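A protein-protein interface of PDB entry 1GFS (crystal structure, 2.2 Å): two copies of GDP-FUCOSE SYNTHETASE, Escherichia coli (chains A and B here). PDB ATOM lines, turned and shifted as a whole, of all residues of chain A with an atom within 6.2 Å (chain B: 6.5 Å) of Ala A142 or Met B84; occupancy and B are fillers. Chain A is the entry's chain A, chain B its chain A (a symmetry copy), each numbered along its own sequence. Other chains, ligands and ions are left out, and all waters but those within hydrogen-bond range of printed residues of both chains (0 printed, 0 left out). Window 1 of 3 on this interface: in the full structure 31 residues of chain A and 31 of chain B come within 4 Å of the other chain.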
ATOM      1  N   MET A  84      -3.704   5.799  15.517  1.00  0.00           N
ATOM      2  CA  MET A  84      -2.904   5.081  14.528  1.00  0.00           C
ATOM      3  C   MET A  84      -3.643   4.990  13.198  1.00  0.00           C
ATOM      4  O   MET A  84      -3.048   5.224  12.153  1.00  0.00           O
ATOM      5  CB  MET A  84      -2.526   3.683  15.019  1.00  0.00           C
ATOM      6  CG  MET A  84      -1.240   3.601  15.850  1.00  0.00           C
ATOM      7  SD  MET A  84      -1.010   1.897  16.503  1.00  0.00           S
ATOM      8  CE  MET A  84      -0.625   0.982  15.012  1.00  0.00           C
ATOM      9  N   MET A  85      -4.933   4.665  13.243  1.00  0.00           N
ATOM     10  CA  MET A  85      -5.742   4.560  12.021  1.00  0.00           C
ATOM     11  C   MET A  85      -5.890   5.892  11.302  1.00  0.00           C
ATOM     12  O   MET A  85      -5.699   5.941  10.096  1.00  0.00           O
ATOM     13  CB  MET A  85      -7.129   3.976  12.280  1.00  0.00           C
ATOM     14  CG  MET A  85      -7.129   2.490  12.545  1.00  0.00           C
ATOM     15  SD  MET A  85      -6.363   1.488  11.249  1.00  0.00           S
ATOM     16  CE  MET A  85      -7.536   1.722   9.924  1.00  0.00           C
ATOM     17  N   GLU A  87      -3.939   8.571  11.409  1.00  0.00           N
ATOM     18  CA  GLU A  87      -2.632   8.922  10.840  1.00  0.00           C
ATOM     19  C   GLU A  87      -2.322   8.144   9.560  1.00  0.00           C
ATOM     20  O   GLU A  87      -2.028   8.742   8.530  1.00  0.00           O
ATOM     21  CB  GLU A  87      -1.526   8.640  11.849  1.00  0.00           C
ATOM     22  CG  GLU A  87      -1.369   9.706  12.886  1.00  0.00           C
ATOM     23  CD  GLU A  87      -0.745   9.182  14.158  1.00  0.00           C
ATOM     24  OE1 GLU A  87      -0.063   8.133  14.119  1.00  0.00           O
ATOM     25  OE2 GLU A  87      -0.974   9.811  15.212  1.00  0.00           O
ATOM     26  N   SER A  88      -2.407   6.813   9.650  1.00  0.00           N
ATOM     27  CA  SER A  88      -2.142   5.881   8.547  1.00  0.00           C
ATOM     28  C   SER A  88      -3.024   6.096   7.334  1.00  0.00           C
ATOM     29  O   SER A  88      -2.539   6.083   6.203  1.00  0.00           O
ATOM     30  CB  SER A  88      -2.331   4.439   9.020  1.00  0.00           C
ATOM     31  OG  SER A  88      -1.392   4.126  10.019  1.00  0.00           O
ATOM     32  N   ILE A  91      -2.235   9.854   5.779  1.00  0.00           N
ATOM     33  CA  ILE A  91      -0.890   9.894   5.203  1.00  0.00           C
ATOM     34  C   ILE A  91      -0.723   8.998   3.973  1.00  0.00           C
ATOM     35  O   ILE A  91      -0.131   9.412   2.979  1.00  0.00           O
ATOM     36  CB  ILE A  91       0.185   9.597   6.272  1.00  0.00           C
ATOM     37  CG1 ILE A  91       0.227  10.744   7.280  1.00  0.00           C
ATOM     38  CG2 ILE A  91       1.549   9.427   5.635  1.00  0.00           C
ATOM     39  CD1 ILE A  91       1.178  10.518   8.440  1.00  0.00           C
ATOM     40  N   PHE A 104       1.802  17.353  10.029  1.00  0.00           N
ATOM     41  CA  PHE A 104       1.287  16.511  11.095  1.00  0.00           C
ATOM     42  C   PHE A 104       1.465  17.225  12.441  1.00  0.00           C
ATOM     43  O   PHE A 104       2.566  17.673  12.770  1.00  0.00           O
ATOM     44  CB  PHE A 104       2.029  15.163  11.083  1.00  0.00           C
ATOM     45  CG  PHE A 104       1.677  14.260  12.227  1.00  0.00           C
ATOM     46  CD1 PHE A 104       0.392  13.749  12.358  1.00  0.00           C
ATOM     47  CD2 PHE A 104       2.636  13.928  13.186  1.00  0.00           C
ATOM     48  CE1 PHE A 104       0.062  12.917  13.428  1.00  0.00           C
ATOM     49  CE2 PHE A 104       2.318  13.097  14.257  1.00  0.00           C
ATOM     50  CZ  PHE A 104       1.029  12.593  14.377  1.00  0.00           C
ATOM     51  N   ALA A 137       1.023   8.559  23.079  1.00  0.00           N
ATOM     52  CA  ALA A 137       2.370   8.944  22.671  1.00  0.00           C
ATOM     53  C   ALA A 137       2.946   8.018  21.602  1.00  0.00           C
ATOM     54  O   ALA A 137       3.587   8.472  20.658  1.00  0.00           O
ATOM     55  CB  ALA A 137       3.291   8.975  23.878  1.00  0.00           C
ATOM     56  N   ILE A 138       2.726   6.721  21.749  1.00  0.00           N
ATOM     57  CA  ILE A 138       3.242   5.769  20.775  1.00  0.00           C
ATOM     58  C   ILE A 138       2.607   6.018  19.416  1.00  0.00           C
ATOM     59  O   ILE A 138       3.284   5.957  18.393  1.00  0.00           O
ATOM     60  CB  ILE A 138       2.992   4.317  21.223  1.00  0.00           C
ATOM     61  CG1 ILE A 138       3.818   4.020  22.475  1.00  0.00           C
ATOM     62  CG2 ILE A 138       3.314   3.344  20.097  1.00  0.00           C
ATOM     63  CD1 ILE A 138       5.310   4.040  22.253  1.00  0.00           C
ATOM     64  N   ALA A 139       1.311   6.314  19.417  1.00  0.00           N
ATOM     65  CA  ALA A 139       0.592   6.590  18.176  1.00  0.00           C
ATOM     66  C   ALA A 139       1.155   7.847  17.496  1.00  0.00           C
ATOM     67  O   ALA A 139       1.371   7.858  16.279  1.00  0.00           O
ATOM     68  CB  ALA A 139      -0.911   6.753  18.451  1.00  0.00           C
ATOM     69  N   LYS A 140       1.422   8.886  18.291  1.00  0.00           N
ATOM     70  CA  LYS A 140       1.958  10.142  17.771  1.00  0.00           C
ATOM     71  C   LYS A 140       3.357   9.968  17.170  1.00  0.00           C
ATOM     72  O   LYS A 140       3.657  10.511  16.106  1.00  0.00           O
ATOM     73  CB  LYS A 140       1.961  11.233  18.859  1.00  0.00           C
ATOM     74  CG  LYS A 140       0.586  11.783  19.185  1.00  0.00           C
ATOM     75  CD  LYS A 140      -0.038  12.330  17.908  1.00  0.00           C
ATOM     76  CE  LYS A 140      -1.370  12.990  18.132  1.00  0.00           C
ATOM     77  NZ  LYS A 140      -1.731  13.784  16.932  1.00  0.00           N
ATOM     78  N   ILE A 141       4.213   9.226  17.867  1.00  0.00           N
ATOM     79  CA  ILE A 141       5.556   8.967  17.386  1.00  0.00           C
ATOM     80  C   ILE A 141       5.464   8.196  16.065  1.00  0.00           C
ATOM     81  O   ILE A 141       6.173   8.526  15.115  1.00  0.00           O
ATOM     82  CB  ILE A 141       6.384   8.192  18.443  1.00  0.00           C
ATOM     83  CG1 ILE A 141       6.720   9.117  19.609  1.00  0.00           C
ATOM     84  CG2 ILE A 141       7.665   7.628  17.837  1.00  0.00           C
ATOM     85  CD1 ILE A 141       7.213   8.381  20.835  1.00  0.00           C
ATOM     86  N   ALA A 142       4.562   7.214  15.987  1.00  0.00           N
ATOM     87  CA  ALA A 142       4.386   6.436  14.758  1.00  0.00           C
ATOM     88  C   ALA A 142       3.968   7.364  13.618  1.00  0.00           C
ATOM     89  O   ALA A 142       4.334   7.129  12.469  1.00  0.00           O
ATOM     90  CB  ALA A 142       3.342   5.347  14.950  1.00  0.00           C
ATOM     91  N   GLY A 143       3.197   8.409  13.947  1.00  0.00           N
ATOM     92  CA  GLY A 143       2.758   9.390  12.960  1.00  0.00           C
ATOM     93  C   GLY A 143       3.944  10.146  12.379  1.00  0.00           C
ATOM     94  O   GLY A 143       4.025  10.350  11.168  1.00  0.00           O
ATOM     95  N   ILE A 144       4.879  10.542  13.243  1.00  0.00           N
ATOM     96  CA  ILE A 144       6.080  11.256  12.819  1.00  0.00           C
ATOM     97  C   ILE A 144       6.943  10.357  11.936  1.00  0.00           C
ATOM     98  O   ILE A 144       7.448  10.797  10.909  1.00  0.00           O
ATOM     99  CB  ILE A 144       6.951  11.721  14.031  1.00  0.00           C
ATOM    100  CG1 ILE A 144       6.224  12.795  14.844  1.00  0.00           C
ATOM    101  CG2 ILE A 144       8.299  12.285  13.547  1.00  0.00           C
ATOM    102  CD1 ILE A 144       6.909  13.081  16.166  1.00  0.00           C
ATOM    103  N   LYS A 145       7.096   9.097  12.329  1.00  0.00           N
ATOM    104  CA  LYS A 145       7.918   8.161  11.574  1.00  0.00           C
ATOM    105  C   LYS A 145       7.312   7.773  10.227  1.00  0.00           C
ATOM    106  O   LYS A 145       8.029   7.381   9.309  1.00  0.00           O
ATOM    107  CB  LYS A 145       8.253   6.937  12.428  1.00  0.00           C
ATOM    108  CG  LYS A 145       9.042   7.290  13.674  1.00  0.00           C
ATOM    109  CD  LYS A 145      10.309   8.033  13.316  1.00  0.00           C
ATOM    110  CE  LYS A 145      11.075   8.529  14.526  1.00  0.00           C
ATOM    111  NZ  LYS A 145      12.261   9.304  14.066  1.00  0.00           N
ATOM    112  N   LEU A 146       5.992   7.849  10.118  1.00  0.00           N
ATOM    113  CA  LEU A 146       5.315   7.568   8.856  1.00  0.00           C
ATOM    114  C   LEU A 146       5.721   8.689   7.901  1.00  0.00           C
ATOM    115  O   LEU A 146       6.128   8.437   6.775  1.00  0.00           O
ATOM    116  CB  LEU A 146       3.800   7.583   9.037  1.00  0.00           C
ATOM    117  CG  LEU A 146       3.111   6.279   9.419  1.00  0.00           C
ATOM    118  CD1 LEU A 146       1.692   6.575   9.871  1.00  0.00           C
ATOM    119  CD2 LEU A 146       3.103   5.335   8.237  1.00  0.00           C
ATOM    120  N   CYS A 147       5.627   9.927   8.380  1.00  0.00           N
ATOM    121  CA  CYS A 147       5.992  11.101   7.592  1.00  0.00           C
ATOM    122  C   CYS A 147       7.421  10.996   7.073  1.00  0.00           C
ATOM    123  O   CYS A 147       7.663  11.156   5.877  1.00  0.00           O
ATOM    124  CB  CYS A 147       5.850  12.389   8.425  1.00  0.00           C
ATOM    125  SG  CYS A 147       4.156  12.936   8.726  1.00  0.00           S
ATOM    126  N   PHE B  79       7.440  -0.616   5.033  1.00  0.00           N
ATOM    127  CA  PHE B  79       7.682  -1.376   6.254  1.00  0.00           C
ATOM    128  C   PHE B  79       6.919  -0.873   7.466  1.00  0.00           C
ATOM    129  O   PHE B  79       6.398  -1.680   8.237  1.00  0.00           O
ATOM    130  CB  PHE B  79       9.170  -1.456   6.569  1.00  0.00           C
ATOM    131  CG  PHE B  79       9.885  -2.530   5.806  1.00  0.00           C
ATOM    132  CD1 PHE B  79      10.322  -2.311   4.506  1.00  0.00           C
ATOM    133  CD2 PHE B  79      10.135  -3.765   6.393  1.00  0.00           C
ATOM    134  CE1 PHE B  79      10.994  -3.306   3.802  1.00  0.00           C
ATOM    135  CE2 PHE B  79      10.810  -4.767   5.694  1.00  0.00           C
ATOM    136  CZ  PHE B  79      11.240  -4.536   4.398  1.00  0.00           C
ATOM    137  N   ILE B  80       6.857   0.444   7.648  1.00  0.00           N
ATOM    138  CA  ILE B  80       6.120   0.979   8.787  1.00  0.00           C
ATOM    139  C   ILE B  80       4.609   0.920   8.548  1.00  0.00           C
ATOM    140  O   ILE B  80       3.866   0.409   9.380  1.00  0.00           O
ATOM    141  CB  ILE B  80       6.587   2.423   9.218  1.00  0.00           C
ATOM    142  CG1 ILE B  80       5.823   2.850  10.473  1.00  0.00           C
ATOM    143  CG2 ILE B  80       6.397   3.450   8.097  1.00  0.00           C
ATOM    144  CD1 ILE B  80       6.410   4.052  11.182  1.00  0.00           C
ATOM    145  N   TYR B  81       4.169   1.362   7.372  1.00  0.00           N
ATOM    146  CA  TYR B  81       2.751   1.359   7.044  1.00  0.00           C
ATOM    147  C   TYR B  81       2.098  -0.029   7.031  1.00  0.00           C
ATOM    148  O   TYR B  81       1.070  -0.251   7.671  1.00  0.00           O
ATOM    149  CB  TYR B  81       2.514   2.049   5.703  1.00  0.00           C
ATOM    150  CG  TYR B  81       1.074   1.938   5.241  1.00  0.00           C
ATOM    151  CD1 TYR B  81       0.094   2.807   5.741  1.00  0.00           C
ATOM    152  CD2 TYR B  81       0.675   0.930   4.347  1.00  0.00           C
ATOM    153  CE1 TYR B  81      -1.245   2.671   5.366  1.00  0.00           C
ATOM    154  CE2 TYR B  81      -0.657   0.791   3.971  1.00  0.00           C
ATOM    155  CZ  TYR B  81      -1.608   1.663   4.486  1.00  0.00           C
ATOM    156  OH  TYR B  81      -2.931   1.524   4.140  1.00  0.00           O
ATOM    157  N   GLN B  82       2.684  -0.965   6.300  1.00  0.00           N
ATOM    158  CA  GLN B  82       2.102  -2.289   6.218  1.00  0.00           C
ATOM    159  C   GLN B  82       2.056  -3.029   7.530  1.00  0.00           C
ATOM    160  O   GLN B  82       1.097  -3.733   7.804  1.00  0.00           O
ATOM    161  CB  GLN B  82       2.806  -3.124   5.156  1.00  0.00           C
ATOM    162  CG  GLN B  82       2.428  -2.728   3.756  1.00  0.00           C
ATOM    163  CD  GLN B  82       3.243  -3.444   2.713  1.00  0.00           C
ATOM    164  OE1 GLN B  82       3.549  -2.882   1.667  1.00  0.00           O
ATOM    165  NE2 GLN B  82       3.617  -4.683   2.993  1.00  0.00           N
ATOM    166  N   ASN B  83       3.111  -2.914   8.325  1.00  0.00           N
ATOM    167  CA  ASN B  83       3.131  -3.586   9.610  1.00  0.00           C
ATOM    168  C   ASN B  83       2.125  -2.944  10.558  1.00  0.00           C
ATOM    169  O   ASN B  83       1.441  -3.650  11.303  1.00  0.00           O
ATOM    170  CB  ASN B  83       4.539  -3.622  10.198  1.00  0.00           C
ATOM    171  CG  ASN B  83       5.421  -4.679   9.524  1.00  0.00           C
ATOM    172  OD1 ASN B  83       5.156  -5.875   9.628  1.00  0.00           O
ATOM    173  ND2 ASN B  83       6.449  -4.236   8.803  1.00  0.00           N
ATOM    174  N   MET B  84       1.979  -1.618  10.484  1.00  0.00           N
ATOM    175  CA  MET B  84       1.007  -0.941  11.339  1.00  0.00           C
ATOM    176  C   MET B  84      -0.414  -1.360  10.983  1.00  0.00           C
ATOM    177  O   MET B  84      -1.208  -1.641  11.872  1.00  0.00           O
ATOM    178  CB  MET B  84       1.148   0.580  11.253  1.00  0.00           C
ATOM    179  CG  MET B  84       2.162   1.205  12.218  1.00  0.00           C
ATOM    180  SD  MET B  84       2.337   3.005  11.881  1.00  0.00           S
ATOM    181  CE  MET B  84       0.757   3.637  12.439  1.00  0.00           C
ATOM    182  N   MET B  85      -0.722  -1.413   9.689  1.00  0.00           N
ATOM    183  CA  MET B  85      -2.060  -1.815   9.236  1.00  0.00           C
ATOM    184  C   MET B  85      -2.386  -3.259   9.584  1.00  0.00           C
ATOM    185  O   MET B  85      -3.465  -3.518  10.097  1.00  0.00           O
ATOM    186  CB  MET B  85      -2.262  -1.606   7.736  1.00  0.00           C
ATOM    187  CG  MET B  85      -2.435  -0.162   7.336  1.00  0.00           C
ATOM    188  SD  MET B  85      -3.781   0.704   8.179  1.00  0.00           S
ATOM    189  CE  MET B  85      -5.192  -0.141   7.486  1.00  0.00           C
ATOM    190  N   ILE B  86      -1.466  -4.189   9.317  1.00  0.00           N
ATOM    191  CA  ILE B  86      -1.679  -5.617   9.628  1.00  0.00           C
ATOM    192  C   ILE B  86      -1.954  -5.812  11.134  1.00  0.00           C
ATOM    193  O   ILE B  86      -2.902  -6.505  11.513  1.00  0.00           O
ATOM    194  CB  ILE B  86      -0.453  -6.491   9.208  1.00  0.00           C
ATOM    195  CG1 ILE B  86      -0.280  -6.476   7.690  1.00  0.00           C
ATOM    196  CG2 ILE B  86      -0.639  -7.941   9.649  1.00  0.00           C
ATOM    197  CD1 ILE B  86       1.020  -7.135   7.230  1.00  0.00           C
ATOM    198  N   GLU B  87      -1.134  -5.182  11.979  1.00  0.00           N
ATOM    199  CA  GLU B  87      -1.306  -5.264  13.434  1.00  0.00           C
ATOM    200  C   GLU B  87      -2.664  -4.734  13.895  1.00  0.00           C
ATOM    201  O   GLU B  87      -3.401  -5.437  14.579  1.00  0.00           O
ATOM    202  CB  GLU B  87      -0.217  -4.464  14.138  1.00  0.00           C
ATOM    203  CG  GLU B  87       1.089  -5.183  14.244  1.00  0.00           C
ATOM    204  CD  GLU B  87       2.258  -4.236  14.372  1.00  0.00           C
ATOM    205  OE1 GLU B  87       2.061  -3.072  14.790  1.00  0.00           O
ATOM    206  OE2 GLU B  87       3.379  -4.655  14.014  1.00  0.00           O
ATOM    207  N   SER B  88      -2.974  -3.496  13.496  1.00  0.00           N
ATOM    208  CA  SER B  88      -4.220  -2.796  13.833  1.00  0.00           C
ATOM    209  C   SER B  88      -5.474  -3.515  13.379  1.00  0.00           C
ATOM    210  O   SER B  88      -6.440  -3.617  14.134  1.00  0.00           O
ATOM    211  CB  SER B  88      -4.224  -1.400  13.210  1.00  0.00           C
ATOM    212  OG  SER B  88      -3.187  -0.619  13.754  1.00  0.00           O
ATOM    213  N   ASN B  89      -5.467  -3.981  12.133  1.00  0.00           N
ATOM    214  CA  ASN B  89      -6.605  -4.695  11.555  1.00  0.00           C
ATOM    215  C   ASN B  89      -6.943  -5.968  12.318  1.00  0.00           C
ATOM    216  O   ASN B  89      -8.064  -6.135  12.778  1.00  0.00           O
ATOM    217  CB  ASN B  89      -6.344  -5.025  10.081  1.00  0.00           C
ATOM    218  CG  ASN B  89      -6.458  -3.811   9.182  1.00  0.00           C
ATOM    219  OD1 ASN B  89      -6.055  -3.848   8.019  1.00  0.00           O
ATOM    220  ND2 ASN B  89      -7.023  -2.729   9.709  1.00  0.00           N
ATOM    221  N   ILE B 138       9.375   0.727  15.047  1.00  0.00           N
ATOM    222  CA  ILE B 138       8.294   1.545  15.582  1.00  0.00           C
ATOM    223  C   ILE B 138       6.964   0.832  15.405  1.00  0.00           C
ATOM    224  O   ILE B 138       6.123   0.854  16.301  1.00  0.00           O
ATOM    225  CB  ILE B 138       8.253   2.928  14.905  1.00  0.00           C
ATOM    226  CG1 ILE B 138       9.508   3.718  15.279  1.00  0.00           C
ATOM    227  CG2 ILE B 138       6.986   3.678  15.293  1.00  0.00           C
ATOM    228  CD1 ILE B 138       9.606   4.072  16.742  1.00  0.00           C
ATOM    229  N   ALA B 139       6.789   0.188  14.256  1.00  0.00           N
ATOM    230  CA  ALA B 139       5.559  -0.548  13.975  1.00  0.00           C
ATOM    231  C   ALA B 139       5.391  -1.712  14.964  1.00  0.00           C
ATOM    232  O   ALA B 139       4.296  -1.930  15.495  1.00  0.00           O
ATOM    233  CB  ALA B 139       5.561  -1.066  12.528  1.00  0.00           C
ATOM    234  N   LYS B 140       6.485  -2.429  15.231  1.00  0.00           N
ATOM    235  CA  LYS B 140       6.462  -3.564  16.152  1.00  0.00           C
ATOM    236  C   LYS B 140       6.130  -3.138  17.585  1.00  0.00           C
ATOM    237  O   LYS B 140       5.347  -3.795  18.272  1.00  0.00           O
ATOM    238  CB  LYS B 140       7.791  -4.341  16.104  1.00  0.00           C
ATOM    239  CG  LYS B 140       7.978  -5.171  14.850  1.00  0.00           C
ATOM    240  CD  LYS B 140       6.810  -6.142  14.728  1.00  0.00           C
ATOM    241  CE  LYS B 140       6.940  -7.086  13.565  1.00  0.00           C
ATOM    242  NZ  LYS B 140       5.967  -8.195  13.724  1.00  0.00           N
ATOM    243  N   ALA B 142       4.481  -0.490  18.422  1.00  0.00           N
ATOM    244  CA  ALA B 142       3.072  -0.085  18.414  1.00  0.00           C
ATOM    245  C   ALA B 142       2.183  -1.322  18.533  1.00  0.00           C
ATOM    246  O   ALA B 142       1.112  -1.254  19.132  1.00  0.00           O
ATOM    247  CB  ALA B 142       2.733   0.677  17.143  1.00  0.00           C
ATOM    248  N   LEU B 146      -0.555  -1.976  21.476  1.00  0.00           N
ATOM    249  CA  LEU B 146      -1.953  -2.185  21.117  1.00  0.00           C
ATOM    250  C   LEU B 146      -2.450  -3.327  22.002  1.00  0.00           C
ATOM    251  O   LEU B 146      -3.495  -3.227  22.630  1.00  0.00           O
ATOM    252  CB  LEU B 146      -2.085  -2.589  19.651  1.00  0.00           C
ATOM    253  CG  LEU B 146      -2.234  -1.484  18.613  1.00  0.00           C
ATOM    254  CD1 LEU B 146      -2.011  -2.062  17.228  1.00  0.00           C
ATOM    255  CD2 LEU B 146      -3.612  -0.867  18.714  1.00  0.00           C
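Of the printed residues of chain B, Ile A138 touches Ala B142. Ile A141 touches none of the printed residues of chain B. Printed residues of chain B within 4 Å of Ala A142: Ile B80 (3.9 Å), Met B84 (3.99 Å) and Ile B138 (3.8 Å). Of the printed residues of chain B, Lys A145 touches Ile B80 (3.6 Å) and Ile B138 (3.9 Å). Of the printed residues of chain B, Leu A146 touches Ile B80 (3.8 Å). Of the printed residues of chain A, Ile B80 touches Ala A142, Lys A145 and Leu A146. Gln B82 touches none of the printed residues of chain A. The nearest printed residue of chain B that does not touch Ala A142 is Ala B142 (5.2 Å). The nearest printed residue of chain A that does not touch Met B84 is Leu A146 (4.01 Å).
O of Met A84 lies within hydrogen-bond range of OG of Ser A88 (2.9 Å). OG of Ser B88 lies within hydrogen-bond range of O of Met B84, 2.9 Å away. OD1 of Asn B89 lies close to O of Met B85, at 3.3 Å.
Among the printed residues, pairs that only touch across the chains: Met A84 with Ser B88 (3.3 Å), Ser A88 with Met B84 (3.3 Å), Lys A145 with Ile B80 (3.6 Å), Ser A88 with Tyr B81 (3.7 Å), Leu A146 with Ile B80 (3.8 Å), Ile A138 with Ala B142 (3.8 Å), Ala A142 with Ile B138 (3.8 Å), Met A85 with Met B85 (3.9 Å), Ala A142 with Ile B80 (3.9 Å), Lys A145 with Ile B138 (3.9 Å), Met A84 with Met B84 (3.9 Å), Met A84 with Ala B142 (3.99 Å) and Ala A142 with Met B84 (3.99 Å).
Of the 17 printed residues of chain A, 7 touch a printed residue of chain B. Of the 16 printed residues of chain B, 7 touch a printed residue of chain A. Along chain B the printed residues that touch a printed residue of chain A span positions 80 to 142. Among the printed residues, 13 pairs touch across the chains. Among the printed residues, no Asp or Glu carboxylate lies within 4 Å of a Lys or Arg side-chain nitrogen of the other chain.
Met B84 touches its own counterpart, Met A84. Met A84 touches Ser B88, and with the chains exchanged Ser A88 touches Met B84. Met A84 touches Ala B142, and with the chains exchanged Ala A142 touches Met B84. Met A85 touches its own counterpart, Met B85. Of the 13 pairs that touch across the chains among the printed residues, 8 have their exchanged pair printed and touching as well.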
